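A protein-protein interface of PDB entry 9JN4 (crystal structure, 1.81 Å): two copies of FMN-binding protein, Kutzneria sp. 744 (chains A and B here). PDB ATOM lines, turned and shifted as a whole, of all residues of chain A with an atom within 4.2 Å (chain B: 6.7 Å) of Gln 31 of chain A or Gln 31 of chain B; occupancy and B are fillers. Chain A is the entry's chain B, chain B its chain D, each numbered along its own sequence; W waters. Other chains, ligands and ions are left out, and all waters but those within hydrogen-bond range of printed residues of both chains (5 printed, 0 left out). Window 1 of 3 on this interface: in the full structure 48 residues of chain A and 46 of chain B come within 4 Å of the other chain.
NE2 of Gln 118 of chain B sits at hydrogen-bond distance from O of Ile 44 of chain A (3.0 Å).
The side-chain amide nitrogen (NE2) of Gln 31 of chain B sits close to the side-chain amide nitrogen (NE2) of Gln 31 of chain A (3.2 Å).
The backbone carbonyl oxygen of Val 88 of chain A sits at hydrogen-bond distance from the backbone NH of Ala 33 of chain A, 2.9 Å away.
N of Gln 31 of chain A sits at hydrogen-bond distance from O of Thr 90 of chain A, 2.8 Å away.
NE2 of Gln 31 of chain B lies close to NE2 of His 46 of chain B (3.4 Å).
O of Thr 90 of chain B is in hydrogen-bond range of N of Gln 31 of chain B (3.0 Å).
O of Val 88 of chain B is in hydrogen-bond range of N of Ala 33 of chain B (2.8 Å).
CG2 of Thr 90 of chain B touches OE1 of Gln 31 of chain A (3.4 Å).
Ala 33 of chain A touches Ile 44 of chain B.
Ala 33 of chain B touches Ile 44 of chain A.
Val 88 of chain B touches Ile 44 of chain A (CG1 to CG1, 3.7 Å).
Ile 44 of chain A touches Thr 90 of chain B.
Ser 116 of chain B touches His 46 of chain A.
CG1 of Ile 44 of chain B touches CG1 of Val 88 of chain A, at 3.6 Å.
Gln 31 of chain B touches Thr 90 of chain A.
Thr 90 of chain A touches Ile 44 of chain B.
CE1 of His 46 of chain B touches CG2 of Thr 90 of chain A (3.96 Å).
Of chain B, only Gln 31 and Thr 90 come within 4 Å of Gln 31 of chain A.
Gln 31 of chain B touches two residues of chain A.
Of the printed residues of chain B, His 46 of chain A touches Ser 116.
Of the printed residues of chain A, Thr 90 of chain B touches Gln 31 and Ile 44.
Ala 92 of chain A touches none of the printed residues of chain B.
Of the 18 printed residues of chain B, 8 touch a printed residue of chain A.
Hydrophobic or aromatic side chains of chain B within 4 Å of the printed part of chain A: Ala 33, Ile 44, His 46 and Val 88.
Among the printed residues, 12 pairs touch across the chains.
Among the printed residues, no Asp or Glu carboxylate lies within 4 Å of a Lys or Arg side-chain nitrogen of the other chain.
Gln 31 of chain A touches its own counterpart, Gln 31 of chain B.
Gln 31 of chain A touches Thr 90 of chain B, and with the chains exchanged Thr 90 of chain A touches Gln 31 of chain B.
Ala 33 of chain A touches Ile 44 of chain B, and with the chains exchanged Ile 44 of chain A touches Ala 33 of chain B.
Ile 44 of chain A touches Thr 90 of chain B, and with the chains exchanged Thr 90 of chain A touches Ile 44 of chain B.
11 positions are printed for both chains.
Of the 12 pairs that touch across the chains among the printed residues, 9 have their exchanged pair printed and touching as well.
Water W5 lies within hydrogen-bond range of the side-chain hydroxyl (OG) of Ser 116 of chain B (2.6 Å), a ring nitrogen (ND1) of His 46 of chain A (2.6 Å) and the side-chain amide nitrogen (NE2) of Gln 118 of chain B (3.1 Å).
Water W1 bridges OE1 of Gln 31 of chain B (2.7 Å) and OE1 of Gln 31 of chain A (2.8 Å).
Water W4 lies within hydrogen-bond range of O of Thr 90 of chain A (2.7 Å) and NE2 of Gln 31 of chain B (2.8 Å).
Water W3 bridges the backbone carbonyl oxygen of Thr 90 of chain B (2.8 Å) and the side-chain amide nitrogen of Gln 31 of chain A (2.9 Å).
Water W2 lies within hydrogen-bond range of N of Ile 44 of chain A (3.1 Å) and OE1 of Gln 118 of chain B (3.2 Å).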
ATOM      1  N   ALA A  30      -0.261  32.104 -32.514  1.00  0.00           N
ATOM      2  CA  ALA A  30       0.871  31.620 -31.706  1.00  0.00           C
ATOM      3  C   ALA A  30       0.896  32.280 -30.345  1.00  0.00           C
ATOM      4  O   ALA A  30       0.337  33.434 -30.171  1.00  0.00           O
ATOM      5  CB  ALA A  30       2.172  31.881 -32.419  1.00  0.00           C
ATOM      6  N   GLN A  31       1.618  31.636 -29.423  1.00  0.00           N
ATOM      7  CA  GLN A  31       1.933  32.283 -28.119  1.00  0.00           C
ATOM      8  C   GLN A  31       3.370  32.795 -28.192  1.00  0.00           C
ATOM      9  O   GLN A  31       4.320  32.005 -28.384  1.00  0.00           O
ATOM     10  CB  GLN A  31       1.748  31.348 -26.922  1.00  0.00           C
ATOM     11  CG  GLN A  31       0.313  30.912 -26.706  1.00  0.00           C
ATOM     12  CD  GLN A  31       0.187  30.069 -25.451  1.00  0.00           C
ATOM     13  OE1 GLN A  31       0.931  30.240 -24.502  1.00  0.00           O
ATOM     14  NE2 GLN A  31      -0.735  29.121 -25.461  1.00  0.00           N
ATOM     15  N   LEU A  32       3.515  34.106 -28.164  1.00  0.00           N
ATOM     16  CA  LEU A  32       4.835  34.763 -28.275  1.00  0.00           C
ATOM     17  C   LEU A  32       5.342  34.984 -26.853  1.00  0.00           C
ATOM     18  O   LEU A  32       4.638  35.633 -26.120  1.00  0.00           O
ATOM     19  CB  LEU A  32       4.691  36.109 -28.991  1.00  0.00           C
ATOM     20  CG  LEU A  32       5.978  36.908 -29.112  1.00  0.00           C
ATOM     21  CD1 LEU A  32       6.962  36.202 -30.031  1.00  0.00           C
ATOM     22  CD2 LEU A  32       5.691  38.319 -29.617  1.00  0.00           C
ATOM     23  N   ALA A  33       6.542  34.506 -26.534  1.00  0.00           N
ATOM     24  CA  ALA A  33       7.116  34.593 -25.180  1.00  0.00           C
ATOM     25  C   ALA A  33       8.469  35.306 -25.256  1.00  0.00           C
ATOM     26  O   ALA A  33       9.302  34.949 -26.095  1.00  0.00           O
ATOM     27  CB  ALA A  33       7.245  33.222 -24.527  1.00  0.00           C
ATOM     28  N   ILE A  44       3.749  36.780 -22.168  1.00  0.00           N
ATOM     29  CA  ILE A  44       3.124  35.858 -23.159  1.00  0.00           C
ATOM     30  C   ILE A  44       1.981  36.605 -23.846  1.00  0.00           C
ATOM     31  O   ILE A  44       1.063  37.145 -23.131  1.00  0.00           O
ATOM     32  CB  ILE A  44       2.576  34.614 -22.445  1.00  0.00           C
ATOM     33  CG1 ILE A  44       3.602  33.897 -21.561  1.00  0.00           C
ATOM     34  CG2 ILE A  44       1.955  33.708 -23.494  1.00  0.00           C
ATOM     35  CD1 ILE A  44       4.479  32.986 -22.371  1.00  0.00           C
ATOM     36  N   THR A  45       2.006  36.685 -25.172  1.00  0.00           N
ATOM     37  CA  THR A  45       0.901  37.312 -25.921  1.00  0.00           C
ATOM     38  C   THR A  45       0.476  36.381 -27.047  1.00  0.00           C
ATOM     39  O   THR A  45       1.401  35.877 -27.702  1.00  0.00           O
ATOM     40  CB  THR A  45       1.304  38.684 -26.470  1.00  0.00           C
ATOM     41  OG1 THR A  45       1.689  39.517 -25.374  1.00  0.00           O
ATOM     42  CG2 THR A  45       0.152  39.310 -27.225  1.00  0.00           C
ATOM     43  N   HIS A  46      -0.845  36.154 -27.222  1.00  0.00           N
ATOM     44  CA  HIS A  46      -1.368  35.459 -28.436  1.00  0.00           C
ATOM     45  C   HIS A  46      -1.373  36.403 -29.632  1.00  0.00           C
ATOM     46  O   HIS A  46      -1.979  37.457 -29.564  1.00  0.00           O
ATOM     47  CB  HIS A  46      -2.743  34.868 -28.260  1.00  0.00           C
ATOM     48  CG  HIS A  46      -2.776  33.605 -27.468  1.00  0.00           C
ATOM     49  ND1 HIS A  46      -2.818  33.625 -26.091  1.00  0.00           N
ATOM     50  CD2 HIS A  46      -2.871  32.307 -27.850  1.00  0.00           C
ATOM     51  CE1 HIS A  46      -2.872  32.382 -25.648  1.00  0.00           C
ATOM     52  NE2 HIS A  46      -2.932  31.547 -26.715  1.00  0.00           N
ATOM     53  N   VAL A  88      10.517  33.200 -28.367  1.00  0.00           N
ATOM     54  CA  VAL A  88       9.991  31.895 -28.831  1.00  0.00           C
ATOM     55  C   VAL A  88       8.556  32.137 -29.232  1.00  0.00           C
ATOM     56  O   VAL A  88       7.847  32.897 -28.510  1.00  0.00           O
ATOM     57  CB  VAL A  88      10.111  30.763 -27.802  1.00  0.00           C
ATOM     58  CG1 VAL A  88       9.485  31.136 -26.466  1.00  0.00           C
ATOM     59  CG2 VAL A  88       9.484  29.496 -28.359  1.00  0.00           C
ATOM     60  N   ALA A  89       8.140  31.593 -30.367  1.00  0.00           N
ATOM     61  CA  ALA A  89       6.681  31.622 -30.670  1.00  0.00           C
ATOM     62  C   ALA A  89       6.256  30.177 -30.785  1.00  0.00           C
ATOM     63  O   ALA A  89       7.006  29.417 -31.454  1.00  0.00           O
ATOM     64  CB  ALA A  89       6.389  32.429 -31.896  1.00  0.00           C
ATOM     65  N   THR A  90       5.222  29.788 -30.035  1.00  0.00           N
ATOM     66  CA  THR A  90       4.743  28.383 -29.934  1.00  0.00           C
ATOM     67  C   THR A  90       3.379  28.305 -30.622  1.00  0.00           C
ATOM     68  O   THR A  90       2.498  29.135 -30.340  1.00  0.00           O
ATOM     69  CB  THR A  90       4.615  27.894 -28.503  1.00  0.00           C
ATOM     70  OG1 THR A  90       5.868  28.193 -27.869  1.00  0.00           O
ATOM     71  CG2 THR A  90       4.250  26.418 -28.409  1.00  0.00           C
ATOM     72  N   ALA A  92       0.276  25.659 -31.482  1.00  0.00           N
ATOM     73  CA  ALA A  92      -0.348  24.489 -30.828  1.00  0.00           C
ATOM     74  C   ALA A  92      -1.365  23.922 -31.821  1.00  0.00           C
ATOM     75  O   ALA A  92      -2.292  24.674 -32.193  1.00  0.00           O
ATOM     76  CB  ALA A  92      -1.001  24.940 -29.512  1.00  0.00           C
ATOM     77  N   PRO B  28      -6.306  21.442 -19.383  1.00  0.00           N
ATOM     78  CA  PRO B  28      -5.228  21.260 -18.407  1.00  0.00           C
ATOM     79  C   PRO B  28      -3.821  21.212 -19.009  1.00  0.00           C
ATOM     80  O   PRO B  28      -2.853  21.301 -18.246  1.00  0.00           O
ATOM     81  CB  PRO B  28      -5.569  19.895 -17.765  1.00  0.00           C
ATOM     82  CG  PRO B  28      -6.369  19.170 -18.810  1.00  0.00           C
ATOM     83  CD  PRO B  28      -7.171  20.256 -19.506  1.00  0.00           C
ATOM     84  N   LEU B  29      -3.718  20.970 -20.317  1.00  0.00           N
ATOM     85  CA  LEU B  29      -2.375  20.884 -20.931  1.00  0.00           C
ATOM     86  C   LEU B  29      -1.902  22.312 -21.211  1.00  0.00           C
ATOM     87  O   LEU B  29      -2.181  22.869 -22.310  1.00  0.00           O
ATOM     88  CB  LEU B  29      -2.369  19.987 -22.167  1.00  0.00           C
ATOM     89  CG  LEU B  29      -0.956  19.679 -22.692  1.00  0.00           C
ATOM     90  CD1 LEU B  29      -0.222  18.710 -21.763  1.00  0.00           C
ATOM     91  CD2 LEU B  29      -0.991  19.148 -24.130  1.00  0.00           C
ATOM     92  N   ALA B  30      -1.178  22.854 -20.239  1.00  0.00           N
ATOM     93  CA  ALA B  30      -0.710  24.248 -20.198  1.00  0.00           C
ATOM     94  C   ALA B  30       0.650  24.348 -20.890  1.00  0.00           C
ATOM     95  O   ALA B  30       1.362  23.360 -20.972  1.00  0.00           O
ATOM     96  CB  ALA B  30      -0.636  24.684 -18.764  1.00  0.00           C
ATOM     97  N   GLN B  31       1.009  25.547 -21.316  1.00  0.00           N
ATOM     98  CA  GLN B  31       2.388  25.865 -21.737  1.00  0.00           C
ATOM     99  C   GLN B  31       3.024  26.531 -20.524  1.00  0.00           C
ATOM    100  O   GLN B  31       2.615  27.692 -20.197  1.00  0.00           O
ATOM    101  CB  GLN B  31       2.332  26.739 -22.998  1.00  0.00           C
ATOM    102  CG  GLN B  31       1.996  25.993 -24.293  1.00  0.00           C
ATOM    103  CD  GLN B  31       2.069  26.840 -25.555  1.00  0.00           C
ATOM    104  OE1 GLN B  31       2.916  27.713 -25.665  1.00  0.00           O
ATOM    105  NE2 GLN B  31       1.086  26.706 -26.435  1.00  0.00           N
ATOM    106  N   LEU B  32       3.965  25.846 -19.909  1.00  0.00           N
ATOM    107  CA  LEU B  32       4.739  26.368 -18.753  1.00  0.00           C
ATOM    108  C   LEU B  32       5.925  27.156 -19.294  1.00  0.00           C
ATOM    109  O   LEU B  32       6.762  26.527 -19.981  1.00  0.00           O
ATOM    110  CB  LEU B  32       5.166  25.202 -17.852  1.00  0.00           C
ATOM    111  CG  LEU B  32       5.973  25.576 -16.591  1.00  0.00           C
ATOM    112  CD1 LEU B  32       5.268  26.618 -15.730  1.00  0.00           C
ATOM    113  CD2 LEU B  32       6.254  24.340 -15.739  1.00  0.00           C
ATOM    114  N   ALA B  33       6.038  28.464 -18.946  1.00  0.00           N
ATOM    115  CA  ALA B  33       7.129  29.310 -19.452  1.00  0.00           C
ATOM    116  C   ALA B  33       8.017  29.748 -18.279  1.00  0.00           C
ATOM    117  O   ALA B  33       7.469  30.236 -17.285  1.00  0.00           O
ATOM    118  CB  ALA B  33       6.613  30.502 -20.240  1.00  0.00           C
ATOM    119  N   ILE B  44       9.805  26.613 -22.862  1.00  0.00           N
ATOM    120  CA  ILE B  44       8.353  26.336 -23.034  1.00  0.00           C
ATOM    121  C   ILE B  44       8.142  24.836 -22.990  1.00  0.00           C
ATOM    122  O   ILE B  44       8.857  24.141 -23.785  1.00  0.00           O
ATOM    123  CB  ILE B  44       7.836  26.906 -24.360  1.00  0.00           C
ATOM    124  CG1 ILE B  44       8.150  28.387 -24.561  1.00  0.00           C
ATOM    125  CG2 ILE B  44       6.373  26.573 -24.501  1.00  0.00           C
ATOM    126  CD1 ILE B  44       7.429  29.330 -23.637  1.00  0.00           C
ATOM    127  N   THR B  45       7.343  24.343 -22.019  1.00  0.00           N
ATOM    128  CA  THR B  45       6.985  22.899 -21.934  1.00  0.00           C
ATOM    129  C   THR B  45       5.473  22.769 -21.814  1.00  0.00           C
ATOM    130  O   THR B  45       4.858  23.429 -20.969  1.00  0.00           O
ATOM    131  CB  THR B  45       7.741  22.169 -20.809  1.00  0.00           C
ATOM    132  OG1 THR B  45       9.147  22.479 -20.960  1.00  0.00           O
ATOM    133  CG2 THR B  45       7.495  20.669 -20.852  1.00  0.00           C
ATOM    134  N   HIS B  46       4.873  21.923 -22.656  1.00  0.00           N
ATOM    135  CA  HIS B  46       3.446  21.552 -22.512  1.00  0.00           C
ATOM    136  C   HIS B  46       3.350  20.587 -21.329  1.00  0.00           C
ATOM    137  O   HIS B  46       3.924  19.512 -21.369  1.00  0.00           O
ATOM    138  CB  HIS B  46       2.846  20.955 -23.785  1.00  0.00           C
ATOM    139  CG  HIS B  46       2.401  21.976 -24.787  1.00  0.00           C
ATOM    140  ND1 HIS B  46       3.258  22.554 -25.690  1.00  0.00           N
ATOM    141  CD2 HIS B  46       1.193  22.506 -25.029  1.00  0.00           C
ATOM    142  CE1 HIS B  46       2.592  23.398 -26.460  1.00  0.00           C
ATOM    143  NE2 HIS B  46       1.333  23.377 -26.084  1.00  0.00           N
ATOM    144  N   VAL B  47       2.654  20.993 -20.284  1.00  0.00           N
ATOM    145  CA  VAL B  47       2.542  20.161 -19.060  1.00  0.00           C
ATOM    146  C   VAL B  47       1.095  20.089 -18.553  1.00  0.00           C
ATOM    147  O   VAL B  47       0.389  21.090 -18.536  1.00  0.00           O
ATOM    148  CB  VAL B  47       3.465  20.700 -17.958  1.00  0.00           C
ATOM    149  CG1 VAL B  47       4.927  20.490 -18.300  1.00  0.00           C
ATOM    150  CG2 VAL B  47       3.203  22.166 -17.688  1.00  0.00           C
ATOM    151  N   ILE B  49      -1.554  20.368 -15.811  1.00  0.00           N
ATOM    152  CA  ILE B  49      -1.673  21.102 -14.541  1.00  0.00           C
ATOM    153  C   ILE B  49      -3.132  21.033 -14.085  1.00  0.00           C
ATOM    154  O   ILE B  49      -4.043  21.270 -14.904  1.00  0.00           O
ATOM    155  CB  ILE B  49      -1.187  22.544 -14.665  1.00  0.00           C
ATOM    156  CG1 ILE B  49       0.318  22.648 -14.938  1.00  0.00           C
ATOM    157  CG2 ILE B  49      -1.586  23.276 -13.396  1.00  0.00           C
ATOM    158  CD1 ILE B  49       0.823  24.048 -15.269  1.00  0.00           C
ATOM    159  N   VAL B  88       5.122  31.493 -15.631  1.00  0.00           N
ATOM    160  CA  VAL B  88       3.733  31.665 -16.124  1.00  0.00           C
ATOM    161  C   VAL B  88       3.279  30.332 -16.702  1.00  0.00           C
ATOM    162  O   VAL B  88       4.075  29.634 -17.342  1.00  0.00           O
ATOM    163  CB  VAL B  88       3.577  32.816 -17.142  1.00  0.00           C
ATOM    164  CG1 VAL B  88       4.620  32.733 -18.245  1.00  0.00           C
ATOM    165  CG2 VAL B  88       2.185  32.835 -17.718  1.00  0.00           C
ATOM    166  N   ALA B  89       2.051  29.958 -16.401  1.00  0.00           N
ATOM    167  CA  ALA B  89       1.401  28.778 -16.998  1.00  0.00           C
ATOM    168  C   ALA B  89       0.210  29.312 -17.789  1.00  0.00           C
ATOM    169  O   ALA B  89      -0.622  30.039 -17.182  1.00  0.00           O
ATOM    170  CB  ALA B  89       0.999  27.784 -15.955  1.00  0.00           C
ATOM    171  N   THR B  90       0.186  29.069 -19.104  1.00  0.00           N
ATOM    172  CA  THR B  90      -0.876  29.581 -20.012  1.00  0.00           C
ATOM    173  C   THR B  90      -1.811  28.432 -20.409  1.00  0.00           C
ATOM    174  O   THR B  90      -1.335  27.376 -20.929  1.00  0.00           O
ATOM    175  CB  THR B  90      -0.309  30.235 -21.273  1.00  0.00           C
ATOM    176  OG1 THR B  90       0.520  31.302 -20.849  1.00  0.00           O
ATOM    177  CG2 THR B  90      -1.415  30.771 -22.160  1.00  0.00           C
ATOM    178  N   PHE B  91      -3.086  28.604 -20.134  1.00  0.00           N
ATOM    179  CA  PHE B  91      -4.148  27.659 -20.539  1.00  0.00           C
ATOM    180  C   PHE B  91      -4.907  28.301 -21.697  1.00  0.00           C
ATOM    181  O   PHE B  91      -5.332  29.464 -21.635  1.00  0.00           O
ATOM    182  CB  PHE B  91      -5.055  27.338 -19.363  1.00  0.00           C
ATOM    183  CG  PHE B  91      -4.336  26.836 -18.134  1.00  0.00           C
ATOM    184  CD1 PHE B  91      -3.608  27.691 -17.331  1.00  0.00           C
ATOM    185  CD2 PHE B  91      -4.374  25.489 -17.782  1.00  0.00           C
ATOM    186  CE1 PHE B  91      -3.002  27.233 -16.188  1.00  0.00           C
ATOM    187  CE2 PHE B  91      -3.808  25.052 -16.594  1.00  0.00           C
ATOM    188  CZ  PHE B  91      -3.040  25.912 -15.852  1.00  0.00           C
ATOM    189  N   ALA B  92      -5.119  27.524 -22.733  1.00  0.00           N
ATOM    190  CA  ALA B  92      -5.741  28.004 -23.971  1.00  0.00           C
ATOM    191  C   ALA B  92      -7.033  27.226 -24.195  1.00  0.00           C
ATOM    192  O   ALA B  92      -6.971  25.984 -24.386  1.00  0.00           O
ATOM    193  CB  ALA B  92      -4.772  27.862 -25.125  1.00  0.00           C
ATOM    194  N   SER B 116      -7.867  32.593 -23.082  1.00  0.00           N
ATOM    195  CA  SER B 116      -6.629  32.167 -22.387  1.00  0.00           C
ATOM    196  C   SER B 116      -6.682  32.506 -20.923  1.00  0.00           C
ATOM    197  O   SER B 116      -7.234  33.550 -20.555  1.00  0.00           O
ATOM    198  CB  SER B 116      -5.344  32.639 -23.055  1.00  0.00           C
ATOM    199  OG  SER B 116      -5.258  34.040 -23.158  1.00  0.00           O
ATOM    200  N   GLN B 118      -3.621  33.011 -18.022  1.00  0.00           N
ATOM    201  CA  GLN B 118      -2.219  33.122 -17.574  1.00  0.00           C
ATOM    202  C   GLN B 118      -2.143  33.209 -16.072  1.00  0.00           C
ATOM    203  O   GLN B 118      -2.730  34.172 -15.465  1.00  0.00           O
ATOM    204  CB  GLN B 118      -1.497  34.274 -18.220  1.00  0.00           C
ATOM    205  CG  GLN B 118      -1.294  34.067 -19.706  1.00  0.00           C
ATOM    206  CD  GLN B 118      -0.636  35.252 -20.357  1.00  0.00           C
ATOM    207  OE1 GLN B 118       0.129  35.953 -19.734  1.00  0.00           O
ATOM    208  NE2 GLN B 118      -0.864  35.406 -21.644  1.00  0.00           N
HETATM  209  O   HOH W   1       3.728  29.877 -24.352  1.00  0.00           O
HETATM  210  O   HOH W   2       1.949  38.520 -20.416  1.00  0.00           O
HETATM  211  O   HOH W   3      -1.706  27.014 -23.640  1.00  0.00           O
HETATM  212  O   HOH W   4       0.474  27.997 -28.881  1.00  0.00           O
HETATM  213  O   HOH W   5      -2.955  34.947 -23.862  1.00  0.00           O
